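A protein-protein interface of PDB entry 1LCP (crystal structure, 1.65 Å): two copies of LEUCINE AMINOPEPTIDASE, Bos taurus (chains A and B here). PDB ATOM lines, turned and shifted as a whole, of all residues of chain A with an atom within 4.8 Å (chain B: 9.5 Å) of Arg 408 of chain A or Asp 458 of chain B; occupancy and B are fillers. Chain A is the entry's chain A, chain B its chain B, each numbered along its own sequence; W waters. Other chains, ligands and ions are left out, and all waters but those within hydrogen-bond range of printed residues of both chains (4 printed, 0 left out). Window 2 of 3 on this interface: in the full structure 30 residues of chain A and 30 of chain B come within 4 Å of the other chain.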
ATOM      1  N   GLU A 404      21.079 -25.154  10.715  1.00  0.00           N
ATOM      2  CA  GLU A 404      21.300 -26.390   9.937  1.00  0.00           C
ATOM      3  C   GLU A 404      20.836 -26.173   8.488  1.00  0.00           C
ATOM      4  O   GLU A 404      21.304 -26.847   7.567  1.00  0.00           O
ATOM      5  CB  GLU A 404      20.551 -27.578  10.569  1.00  0.00           C
ATOM      6  CG  GLU A 404      20.741 -28.942   9.852  1.00  0.00           C
ATOM      7  CD  GLU A 404      19.785 -29.177   8.673  1.00  0.00           C
ATOM      8  OE1 GLU A 404      18.779 -28.448   8.530  1.00  0.00           O
ATOM      9  OE2 GLU A 404      20.033 -30.107   7.873  1.00  0.00           O
ATOM     10  N   HIS A 405      19.876 -25.266   8.308  1.00  0.00           N
ATOM     11  CA  HIS A 405      19.352 -24.889   6.987  1.00  0.00           C
ATOM     12  C   HIS A 405      20.529 -24.624   6.024  1.00  0.00           C
ATOM     13  O   HIS A 405      20.509 -25.042   4.858  1.00  0.00           O
ATOM     14  CB  HIS A 405      18.494 -23.614   7.159  1.00  0.00           C
ATOM     15  CG  HIS A 405      18.065 -22.961   5.882  1.00  0.00           C
ATOM     16  ND1 HIS A 405      16.743 -22.908   5.475  1.00  0.00           N
ATOM     17  CD2 HIS A 405      18.764 -22.252   4.953  1.00  0.00           C
ATOM     18  CE1 HIS A 405      16.650 -22.200   4.369  1.00  0.00           C
ATOM     19  NE2 HIS A 405      17.853 -21.788   4.028  1.00  0.00           N
ATOM     20  N   TYR A 406      21.554 -23.941   6.532  1.00  0.00           N
ATOM     21  CA  TYR A 406      22.724 -23.607   5.725  1.00  0.00           C
ATOM     22  C   TYR A 406      23.695 -24.794   5.600  1.00  0.00           C
ATOM     23  O   TYR A 406      24.253 -25.038   4.521  1.00  0.00           O
ATOM     24  CB  TYR A 406      23.415 -22.357   6.303  1.00  0.00           C
ATOM     25  CG  TYR A 406      22.488 -21.141   6.416  1.00  0.00           C
ATOM     26  CD1 TYR A 406      21.949 -20.529   5.273  1.00  0.00           C
ATOM     27  CD2 TYR A 406      22.125 -20.627   7.665  1.00  0.00           C
ATOM     28  CE1 TYR A 406      21.060 -19.436   5.373  1.00  0.00           C
ATOM     29  CE2 TYR A 406      21.244 -19.542   7.780  1.00  0.00           C
ATOM     30  CZ  TYR A 406      20.713 -18.953   6.633  1.00  0.00           C
ATOM     31  OH  TYR A 406      19.827 -17.902   6.751  1.00  0.00           O
ATOM     32  N   THR A 407      23.854 -25.548   6.688  1.00  0.00           N
ATOM     33  CA  THR A 407      24.732 -26.726   6.717  1.00  0.00           C
ATOM     34  C   THR A 407      24.306 -27.720   5.626  1.00  0.00           C
ATOM     35  O   THR A 407      25.139 -28.260   4.888  1.00  0.00           O
ATOM     36  CB  THR A 407      24.646 -27.438   8.100  1.00  0.00           C
ATOM     37  OG1 THR A 407      25.036 -26.525   9.137  1.00  0.00           O
ATOM     38  CG2 THR A 407      25.554 -28.680   8.160  1.00  0.00           C
ATOM     39  N   ARG A 408      22.999 -27.931   5.505  1.00  0.00           N
ATOM     40  CA  ARG A 408      22.448 -28.859   4.521  1.00  0.00           C
ATOM     41  C   ARG A 408      22.939 -28.565   3.094  1.00  0.00           C
ATOM     42  O   ARG A 408      23.205 -29.486   2.315  1.00  0.00           O
ATOM     43  CB  ARG A 408      20.913 -28.810   4.570  1.00  0.00           C
ATOM     44  CG  ARG A 408      20.218 -29.872   3.717  1.00  0.00           C
ATOM     45  CD  ARG A 408      18.692 -29.732   3.777  1.00  0.00           C
ATOM     46  NE  ARG A 408      18.033 -30.685   2.886  1.00  0.00           N
ATOM     47  CZ  ARG A 408      16.857 -30.480   2.294  1.00  0.00           C
ATOM     48  NH1 ARG A 408      16.202 -29.336   2.466  1.00  0.00           N
ATOM     49  NH2 ARG A 408      16.347 -31.415   1.505  1.00  0.00           N
ATOM     50  N   GLN A 409      23.122 -27.285   2.778  1.00  0.00           N
ATOM     51  CA  GLN A 409      23.549 -26.879   1.446  1.00  0.00           C
ATOM     52  C   GLN A 409      25.035 -27.065   1.155  1.00  0.00           C
ATOM     53  O   GLN A 409      25.457 -26.947  -0.010  1.00  0.00           O
ATOM     54  CB  GLN A 409      23.079 -25.446   1.149  1.00  0.00           C
ATOM     55  CG  GLN A 409      21.552 -25.330   1.237  1.00  0.00           C
ATOM     56  CD  GLN A 409      20.994 -23.927   1.035  1.00  0.00           C
ATOM     57  OE1 GLN A 409      19.804 -23.680   1.315  1.00  0.00           O
ATOM     58  NE2 GLN A 409      21.821 -23.010   0.543  1.00  0.00           N
ATOM     59  N   VAL A 410      25.832 -27.325   2.190  1.00  0.00           N
ATOM     60  CA  VAL A 410      27.258 -27.558   1.983  1.00  0.00           C
ATOM     61  C   VAL A 410      27.611 -29.040   2.154  1.00  0.00           C
ATOM     62  O   VAL A 410      28.619 -29.504   1.617  1.00  0.00           O
ATOM     63  CB  VAL A 410      28.171 -26.649   2.854  1.00  0.00           C
ATOM     64  CG1 VAL A 410      27.887 -25.175   2.553  1.00  0.00           C
ATOM     65  CG2 VAL A 410      27.995 -26.944   4.324  1.00  0.00           C
ATOM     66  N   ILE A 411      26.797 -29.796   2.888  1.00  0.00           N
ATOM     67  CA  ILE A 411      27.096 -31.220   3.016  1.00  0.00           C
ATOM     68  C   ILE A 411      26.485 -32.005   1.851  1.00  0.00           C
ATOM     69  O   ILE A 411      26.782 -33.182   1.669  1.00  0.00           O
ATOM     70  CB  ILE A 411      26.761 -31.845   4.407  1.00  0.00           C
ATOM     71  CG1 ILE A 411      25.274 -31.783   4.719  1.00  0.00           C
ATOM     72  CG2 ILE A 411      27.571 -31.159   5.495  1.00  0.00           C
ATOM     73  CD1 ILE A 411      24.940 -32.485   6.032  1.00  0.00           C
ATOM     74  N   ASP A 412      25.622 -31.347   1.074  1.00  0.00           N
ATOM     75  CA  ASP A 412      25.045 -31.956  -0.132  1.00  0.00           C
ATOM     76  C   ASP A 412      26.250 -31.831  -1.070  1.00  0.00           C
ATOM     77  O   ASP A 412      26.549 -30.742  -1.573  1.00  0.00           O
ATOM     78  CB  ASP A 412      23.879 -31.103  -0.651  1.00  0.00           C
ATOM     79  CG  ASP A 412      23.169 -31.729  -1.842  1.00  0.00           C
ATOM     80  OD1 ASP A 412      23.766 -32.559  -2.557  1.00  0.00           O
ATOM     81  OD2 ASP A 412      21.988 -31.384  -2.070  1.00  0.00           O
ATOM     82  N   LYS A 423      25.287 -24.885  -2.752  1.00  0.00           N
ATOM     83  CA  LYS A 423      24.580 -25.227  -3.970  1.00  0.00           C
ATOM     84  C   LYS A 423      23.873 -24.030  -4.617  1.00  0.00           C
ATOM     85  O   LYS A 423      23.399 -24.140  -5.746  1.00  0.00           O
ATOM     86  CB  LYS A 423      23.596 -26.391  -3.722  1.00  0.00           C
ATOM     87  CG  LYS A 423      22.834 -26.355  -2.414  1.00  0.00           C
ATOM     88  CD  LYS A 423      22.437 -27.772  -2.006  1.00  0.00           C
ATOM     89  CE  LYS A 423      21.350 -28.349  -2.892  1.00  0.00           C
ATOM     90  NZ  LYS A 423      20.010 -27.761  -2.592  1.00  0.00           N
ATOM     91  N   LYS B  50      10.659 -39.123   7.731  1.00  0.00           N
ATOM     92  CA  LYS B  50      10.625 -40.238   6.775  1.00  0.00           C
ATOM     93  C   LYS B  50       9.269 -40.941   6.855  1.00  0.00           C
ATOM     94  O   LYS B  50       8.576 -40.828   7.866  1.00  0.00           O
ATOM     95  CB  LYS B  50      11.750 -41.250   7.064  1.00  0.00           C
ATOM     96  CG  LYS B  50      13.133 -40.631   7.304  1.00  0.00           C
ATOM     97  CD  LYS B  50      13.648 -39.817   6.120  1.00  0.00           C
ATOM     98  CE  LYS B  50      14.051 -40.684   4.949  1.00  0.00           C
ATOM     99  NZ  LYS B  50      14.579 -39.872   3.805  1.00  0.00           N
ATOM    100  N   GLU B  80      18.497 -23.065  17.058  1.00  0.00           N
ATOM    101  CA  GLU B  80      17.727 -22.830  15.841  1.00  0.00           C
ATOM    102  C   GLU B  80      16.613 -21.793  15.964  1.00  0.00           C
ATOM    103  O   GLU B  80      16.016 -21.399  14.959  1.00  0.00           O
ATOM    104  CB  GLU B  80      17.156 -24.157  15.326  1.00  0.00           C
ATOM    105  CG  GLU B  80      18.214 -25.215  14.974  1.00  0.00           C
ATOM    106  CD  GLU B  80      18.939 -24.949  13.659  1.00  0.00           C
ATOM    107  OE1 GLU B  80      18.465 -24.120  12.858  1.00  0.00           O
ATOM    108  OE2 GLU B  80      19.992 -25.586  13.423  1.00  0.00           O
ATOM    109  N   GLU B  87       8.020 -28.296  14.332  1.00  0.00           N
ATOM    110  CA  GLU B  87       8.609 -28.391  12.999  1.00  0.00           C
ATOM    111  C   GLU B  87       8.677 -29.854  12.534  1.00  0.00           C
ATOM    112  O   GLU B  87       8.435 -30.150  11.355  1.00  0.00           O
ATOM    113  CB  GLU B  87      10.004 -27.739  12.952  1.00  0.00           C
ATOM    114  CG  GLU B  87       9.964 -26.229  12.700  1.00  0.00           C
ATOM    115  CD  GLU B  87       9.467 -25.858  11.296  1.00  0.00           C
ATOM    116  OE1 GLU B  87      10.120 -26.235  10.301  1.00  0.00           O
ATOM    117  OE2 GLU B  87       8.431 -25.167  11.187  1.00  0.00           O
ATOM    118  N   ALA B  91       6.607 -31.293   9.137  1.00  0.00           N
ATOM    119  CA  ALA B  91       7.311 -31.998   8.066  1.00  0.00           C
ATOM    120  C   ALA B  91       6.814 -33.434   7.859  1.00  0.00           C
ATOM    121  O   ALA B  91       6.508 -33.833   6.733  1.00  0.00           O
ATOM    122  CB  ALA B  91       8.808 -31.996   8.331  1.00  0.00           C
ATOM    123  N   ARG B  98       1.426 -36.349   1.258  1.00  0.00           N
ATOM    124  CA  ARG B  98       1.882 -36.390  -0.133  1.00  0.00           C
ATOM    125  C   ARG B  98       1.880 -37.829  -0.657  1.00  0.00           C
ATOM    126  O   ARG B  98       1.559 -38.062  -1.829  1.00  0.00           O
ATOM    127  CB  ARG B  98       3.278 -35.760  -0.302  1.00  0.00           C
ATOM    128  CG  ARG B  98       3.320 -34.229  -0.086  1.00  0.00           C
ATOM    129  CD  ARG B  98       4.639 -33.595  -0.572  1.00  0.00           C
ATOM    130  NE  ARG B  98       5.827 -34.310  -0.087  1.00  0.00           N
ATOM    131  CZ  ARG B  98       6.567 -33.945   0.961  1.00  0.00           C
ATOM    132  NH1 ARG B  98       6.261 -32.846   1.653  1.00  0.00           N
ATOM    133  NH2 ARG B  98       7.617 -34.681   1.312  1.00  0.00           N
ATOM    134  N   SER B 370      16.822 -17.992   2.228  1.00  0.00           N
ATOM    135  CA  SER B 370      15.496 -18.394   2.720  1.00  0.00           C
ATOM    136  C   SER B 370      15.495 -18.850   4.191  1.00  0.00           C
ATOM    137  O   SER B 370      14.507 -19.402   4.690  1.00  0.00           O
ATOM    138  CB  SER B 370      14.928 -19.506   1.831  1.00  0.00           C
ATOM    139  OG  SER B 370      15.819 -20.614   1.802  1.00  0.00           O
ATOM    140  N   THR B 455      10.370 -17.594  -2.291  1.00  0.00           N
ATOM    141  CA  THR B 455      10.151 -18.926  -2.858  1.00  0.00           C
ATOM    142  C   THR B 455      10.685 -20.060  -2.000  1.00  0.00           C
ATOM    143  O   THR B 455      11.472 -19.839  -1.067  1.00  0.00           O
ATOM    144  CB  THR B 455      10.873 -19.085  -4.237  1.00  0.00           C
ATOM    145  OG1 THR B 455      12.289 -19.257  -4.029  1.00  0.00           O
ATOM    146  CG2 THR B 455      10.634 -17.876  -5.147  1.00  0.00           C
ATOM    147  N   ASN B 456      10.263 -21.275  -2.351  1.00  0.00           N
ATOM    148  CA  ASN B 456      10.729 -22.485  -1.705  1.00  0.00           C
ATOM    149  C   ASN B 456      11.092 -23.501  -2.786  1.00  0.00           C
ATOM    150  O   ASN B 456      10.438 -23.590  -3.828  1.00  0.00           O
ATOM    151  CB  ASN B 456       9.662 -23.121  -0.792  1.00  0.00           C
ATOM    152  CG  ASN B 456      10.254 -24.192   0.134  1.00  0.00           C
ATOM    153  OD1 ASN B 456       9.938 -25.386   0.038  1.00  0.00           O
ATOM    154  ND2 ASN B 456      11.132 -23.763   1.025  1.00  0.00           N
ATOM    155  N   LYS B 457      12.212 -24.179  -2.568  1.00  0.00           N
ATOM    156  CA  LYS B 457      12.671 -25.270  -3.428  1.00  0.00           C
ATOM    157  C   LYS B 457      12.319 -26.454  -2.521  1.00  0.00           C
ATOM    158  O   LYS B 457      11.265 -27.068  -2.694  1.00  0.00           O
ATOM    159  CB  LYS B 457      14.171 -25.145  -3.720  1.00  0.00           C
ATOM    160  CG  LYS B 457      14.470 -24.027  -4.725  1.00  0.00           C
ATOM    161  CD  LYS B 457      15.959 -23.881  -5.036  1.00  0.00           C
ATOM    162  CE  LYS B 457      16.648 -22.914  -4.076  1.00  0.00           C
ATOM    163  NZ  LYS B 457      16.202 -21.514  -4.281  1.00  0.00           N
ATOM    164  N   ASP B 458      13.148 -26.740  -1.520  1.00  0.00           N
ATOM    165  CA  ASP B 458      12.809 -27.791  -0.560  1.00  0.00           C
ATOM    166  C   ASP B 458      13.360 -27.508   0.846  1.00  0.00           C
ATOM    167  O   ASP B 458      13.367 -28.392   1.714  1.00  0.00           O
ATOM    168  CB  ASP B 458      13.197 -29.190  -1.073  1.00  0.00           C
ATOM    169  CG  ASP B 458      14.675 -29.498  -0.937  1.00  0.00           C
ATOM    170  OD1 ASP B 458      15.513 -28.569  -0.893  1.00  0.00           O
ATOM    171  OD2 ASP B 458      15.004 -30.699  -0.872  1.00  0.00           O
ATOM    172  N   GLU B 459      13.754 -26.258   1.093  1.00  0.00           N
ATOM    173  CA  GLU B 459      14.313 -25.863   2.384  1.00  0.00           C
ATOM    174  C   GLU B 459      13.312 -26.077   3.530  1.00  0.00           C
ATOM    175  O   GLU B 459      13.687 -26.527   4.616  1.00  0.00           O
ATOM    176  CB  GLU B 459      14.786 -24.410   2.348  1.00  0.00           C
ATOM    177  CG  GLU B 459      15.757 -24.078   1.208  1.00  0.00           C
ATOM    178  CD  GLU B 459      15.075 -23.410   0.027  1.00  0.00           C
ATOM    179  OE1 GLU B 459      14.098 -23.975  -0.511  1.00  0.00           O
ATOM    180  OE2 GLU B 459      15.519 -22.306  -0.363  1.00  0.00           O
ATOM    181  N   VAL B 460      12.066 -25.662   3.321  1.00  0.00           N
ATOM    182  CA  VAL B 460      10.992 -25.854   4.297  1.00  0.00           C
ATOM    183  C   VAL B 460      10.334 -27.140   3.755  1.00  0.00           C
ATOM    184  O   VAL B 460       9.665 -27.111   2.718  1.00  0.00           O
ATOM    185  CB  VAL B 460       9.992 -24.669   4.288  1.00  0.00           C
ATOM    186  CG1 VAL B 460       8.830 -24.959   5.235  1.00  0.00           C
ATOM    187  CG2 VAL B 460      10.694 -23.388   4.718  1.00  0.00           C
ATOM    188  N   PRO B 461      10.485 -28.270   4.472  1.00  0.00           N
ATOM    189  CA  PRO B 461       9.934 -29.570   4.060  1.00  0.00           C
ATOM    190  C   PRO B 461       8.458 -29.627   3.712  1.00  0.00           C
ATOM    191  O   PRO B 461       8.057 -30.358   2.802  1.00  0.00           O
ATOM    192  CB  PRO B 461      10.242 -30.474   5.258  1.00  0.00           C
ATOM    193  CG  PRO B 461      11.441 -29.843   5.873  1.00  0.00           C
ATOM    194  CD  PRO B 461      11.077 -28.374   5.817  1.00  0.00           C
ATOM    195  N   TYR B 462       7.656 -28.882   4.456  1.00  0.00           N
ATOM    196  CA  TYR B 462       6.205 -28.882   4.257  1.00  0.00           C
ATOM    197  C   TYR B 462       5.624 -27.928   3.214  1.00  0.00           C
ATOM    198  O   TYR B 462       4.406 -27.726   3.175  1.00  0.00           O
ATOM    199  CB  TYR B 462       5.479 -28.749   5.607  1.00  0.00           C
ATOM    200  CG  TYR B 462       5.972 -27.617   6.482  1.00  0.00           C
ATOM    201  CD1 TYR B 462       7.027 -27.803   7.383  1.00  0.00           C
ATOM    202  CD2 TYR B 462       5.387 -26.345   6.407  1.00  0.00           C
ATOM    203  CE1 TYR B 462       7.491 -26.743   8.191  1.00  0.00           C
ATOM    204  CE2 TYR B 462       5.836 -25.285   7.206  1.00  0.00           C
ATOM    205  CZ  TYR B 462       6.882 -25.489   8.095  1.00  0.00           C
ATOM    206  OH  TYR B 462       7.276 -24.445   8.892  1.00  0.00           O
ATOM    207  N   LEU B 463       6.476 -27.322   2.388  1.00  0.00           N
ATOM    208  CA  LEU B 463       5.996 -26.446   1.314  1.00  0.00           C
ATOM    209  C   LEU B 463       6.542 -27.012  -0.006  1.00  0.00           C
ATOM    210  O   LEU B 463       7.742 -27.254  -0.114  1.00  0.00           O
ATOM    211  CB  LEU B 463       6.506 -25.009   1.494  1.00  0.00           C
ATOM    212  CG  LEU B 463       6.120 -24.248   2.767  1.00  0.00           C
ATOM    213  CD1 LEU B 463       6.797 -22.873   2.766  1.00  0.00           C
ATOM    214  CD2 LEU B 463       4.596 -24.083   2.840  1.00  0.00           C
ATOM    215  N   ARG B 464       5.681 -27.291  -0.981  1.00  0.00           N
ATOM    216  CA  ARG B 464       6.159 -27.796  -2.270  1.00  0.00           C
ATOM    217  C   ARG B 464       6.889 -26.651  -2.976  1.00  0.00           C
ATOM    218  O   ARG B 464       6.843 -25.509  -2.507  1.00  0.00           O
ATOM    219  CB  ARG B 464       4.989 -28.303  -3.118  1.00  0.00           C
ATOM    220  CG  ARG B 464       4.542 -29.717  -2.755  1.00  0.00           C
ATOM    221  CD  ARG B 464       3.197 -30.071  -3.389  1.00  0.00           C
ATOM    222  NE  ARG B 464       3.030 -31.523  -3.513  1.00  0.00           N
ATOM    223  CZ  ARG B 464       1.865 -32.167  -3.493  1.00  0.00           C
ATOM    224  NH1 ARG B 464       0.730 -31.499  -3.335  1.00  0.00           N
ATOM    225  NH2 ARG B 464       1.842 -33.496  -3.620  1.00  0.00           N
ATOM    226  N   LYS B 465       7.579 -26.955  -4.070  1.00  0.00           N
ATOM    227  CA  LYS B 465       8.322 -25.944  -4.830  1.00  0.00           C
ATOM    228  C   LYS B 465       7.386 -24.854  -5.379  1.00  0.00           C
ATOM    229  O   LYS B 465       6.357 -25.164  -5.981  1.00  0.00           O
ATOM    230  CB  LYS B 465       9.087 -26.616  -5.979  1.00  0.00           C
ATOM    231  CG  LYS B 465       9.901 -25.656  -6.822  1.00  0.00           C
ATOM    232  CD  LYS B 465      10.554 -26.381  -7.995  1.00  0.00           C
ATOM    233  CE  LYS B 465      11.317 -25.407  -8.884  1.00  0.00           C
ATOM    234  NZ  LYS B 465      12.363 -24.647  -8.126  1.00  0.00           N
ATOM    235  N   GLY B 466       7.743 -23.586  -5.161  1.00  0.00           N
ATOM    236  CA  GLY B 466       6.922 -22.480  -5.635  1.00  0.00           C
ATOM    237  C   GLY B 466       6.938 -21.312  -4.665  1.00  0.00           C
ATOM    238  O   GLY B 466       7.795 -21.255  -3.780  1.00  0.00           O
ATOM    239  N   ALA B 468       6.260 -19.136  -1.532  1.00  0.00           N
ATOM    240  CA  ALA B 468       6.124 -19.587  -0.153  1.00  0.00           C
ATOM    241  C   ALA B 468       5.068 -18.966   0.771  1.00  0.00           C
ATOM    242  O   ALA B 468       4.602 -19.628   1.704  1.00  0.00           O
ATOM    243  CB  ALA B 468       7.510 -19.559   0.521  1.00  0.00           C
ATOM    244  N   ARG B 470       5.554 -16.738   2.924  1.00  0.00           N
ATOM    245  CA  ARG B 470       6.217 -16.498   4.212  1.00  0.00           C
ATOM    246  C   ARG B 470       6.348 -14.978   4.366  1.00  0.00           C
ATOM    247  O   ARG B 470       6.627 -14.274   3.391  1.00  0.00           O
ATOM    248  CB  ARG B 470       7.592 -17.178   4.226  1.00  0.00           C
ATOM    249  CG  ARG B 470       7.533 -18.699   4.082  1.00  0.00           C
ATOM    250  CD  ARG B 470       8.930 -19.335   3.953  1.00  0.00           C
ATOM    251  NE  ARG B 470       9.796 -19.013   5.089  1.00  0.00           N
ATOM    252  CZ  ARG B 470      11.109 -19.250   5.133  1.00  0.00           C
ATOM    253  NH1 ARG B 470      11.730 -19.805   4.093  1.00  0.00           N
ATOM    254  NH2 ARG B 470      11.809 -18.914   6.218  1.00  0.00           N
HETATM  255  O   HOH W   1      17.791 -24.811  10.304  1.00  0.00           O
HETATM  256  O   HOH W   2      18.070 -21.484  -0.412  1.00  0.00           O
HETATM  257  O   HOH W   3      18.965 -20.266   1.797  1.00  0.00           O
HETATM  258  O   HOH W   4      16.294 -27.436   4.808  1.00  0.00           O
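The backbone NH of Glu 404 of chain A lies within hydrogen-bond range of the side-chain carboxylate of Glu 80 of chain B (2.9 Å).
NE2 of His 405 of chain A sits close to OG of Ser 370 of chain B, at 3.2 Å.
OD2 of Asp 458 of chain B lies within salt-bridge range of NH2 of Arg 408 of chain A (2.8 Å).
The side-chain carboxylate (OE2) of Glu 459 of chain B sits at hydrogen-bond distance from the side-chain hydroxyl (OG) of Ser 370 of chain B, at 2.8 Å.
NH1 of Arg 470 of chain B is in hydrogen-bond range of O of Ser 370 of chain B (2.9 Å).
ND2 of Asn 456 of chain B is in hydrogen-bond range of OE1 of Glu 459 of chain B, at 3.3 Å.
OE1 of Glu 459 of chain B is in hydrogen-bond range of N of Lys 457 of chain B.
CE1 of His 405 of chain A touches CB of Glu 459 of chain B (3.5 Å).
Arg 408 of chain A touches Glu 459 of chain B.
Of the printed residues of chain B, Arg 408 of chain A touches Asp 458 (2.8 Å) and Glu 459 (3.95 Å).
Of the printed residues of chain A, Glu 80 of chain B touches Glu 404.
Printed residues of chain A within 4 Å of Ser 370 of chain B: His 405.
Val 460 of chain B touches none of the printed residues of chain A.
The nearest printed residue of chain B that does not touch Glu 404 of chain A is Glu 459 of chain B (6.7 Å).
Of the 10 printed residues of chain A, 3 touch a printed residue of chain B.
Among the printed residues, 5 pairs touch across the chains.
No position is printed for both chains.
Water W2 lies within hydrogen-bond range of the side-chain carboxylate (OE2) of Glu 459 of chain B, the side-chain hydroxyl (OG) of Ser 370 of chain B and the side-chain amide oxygen (OE1) of Gln 409 of chain A.
Water W1 lies within hydrogen-bond range of OE1 of Glu 80 of chain B, N of His 405 of chain A and N of Glu 404 of chain A.
Water W4 lies within hydrogen-bond range of the backbone carbonyl oxygen (O) of Glu 459 of chain B (2.8 Å) and the guanidinium group (NH1) of Arg 408 of chain A (3.0 Å).
Water W3 lies within hydrogen-bond range of NE2 of His 405 of chain A (2.9 Å) and N of Ser 370 of chain B (3.2 Å).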
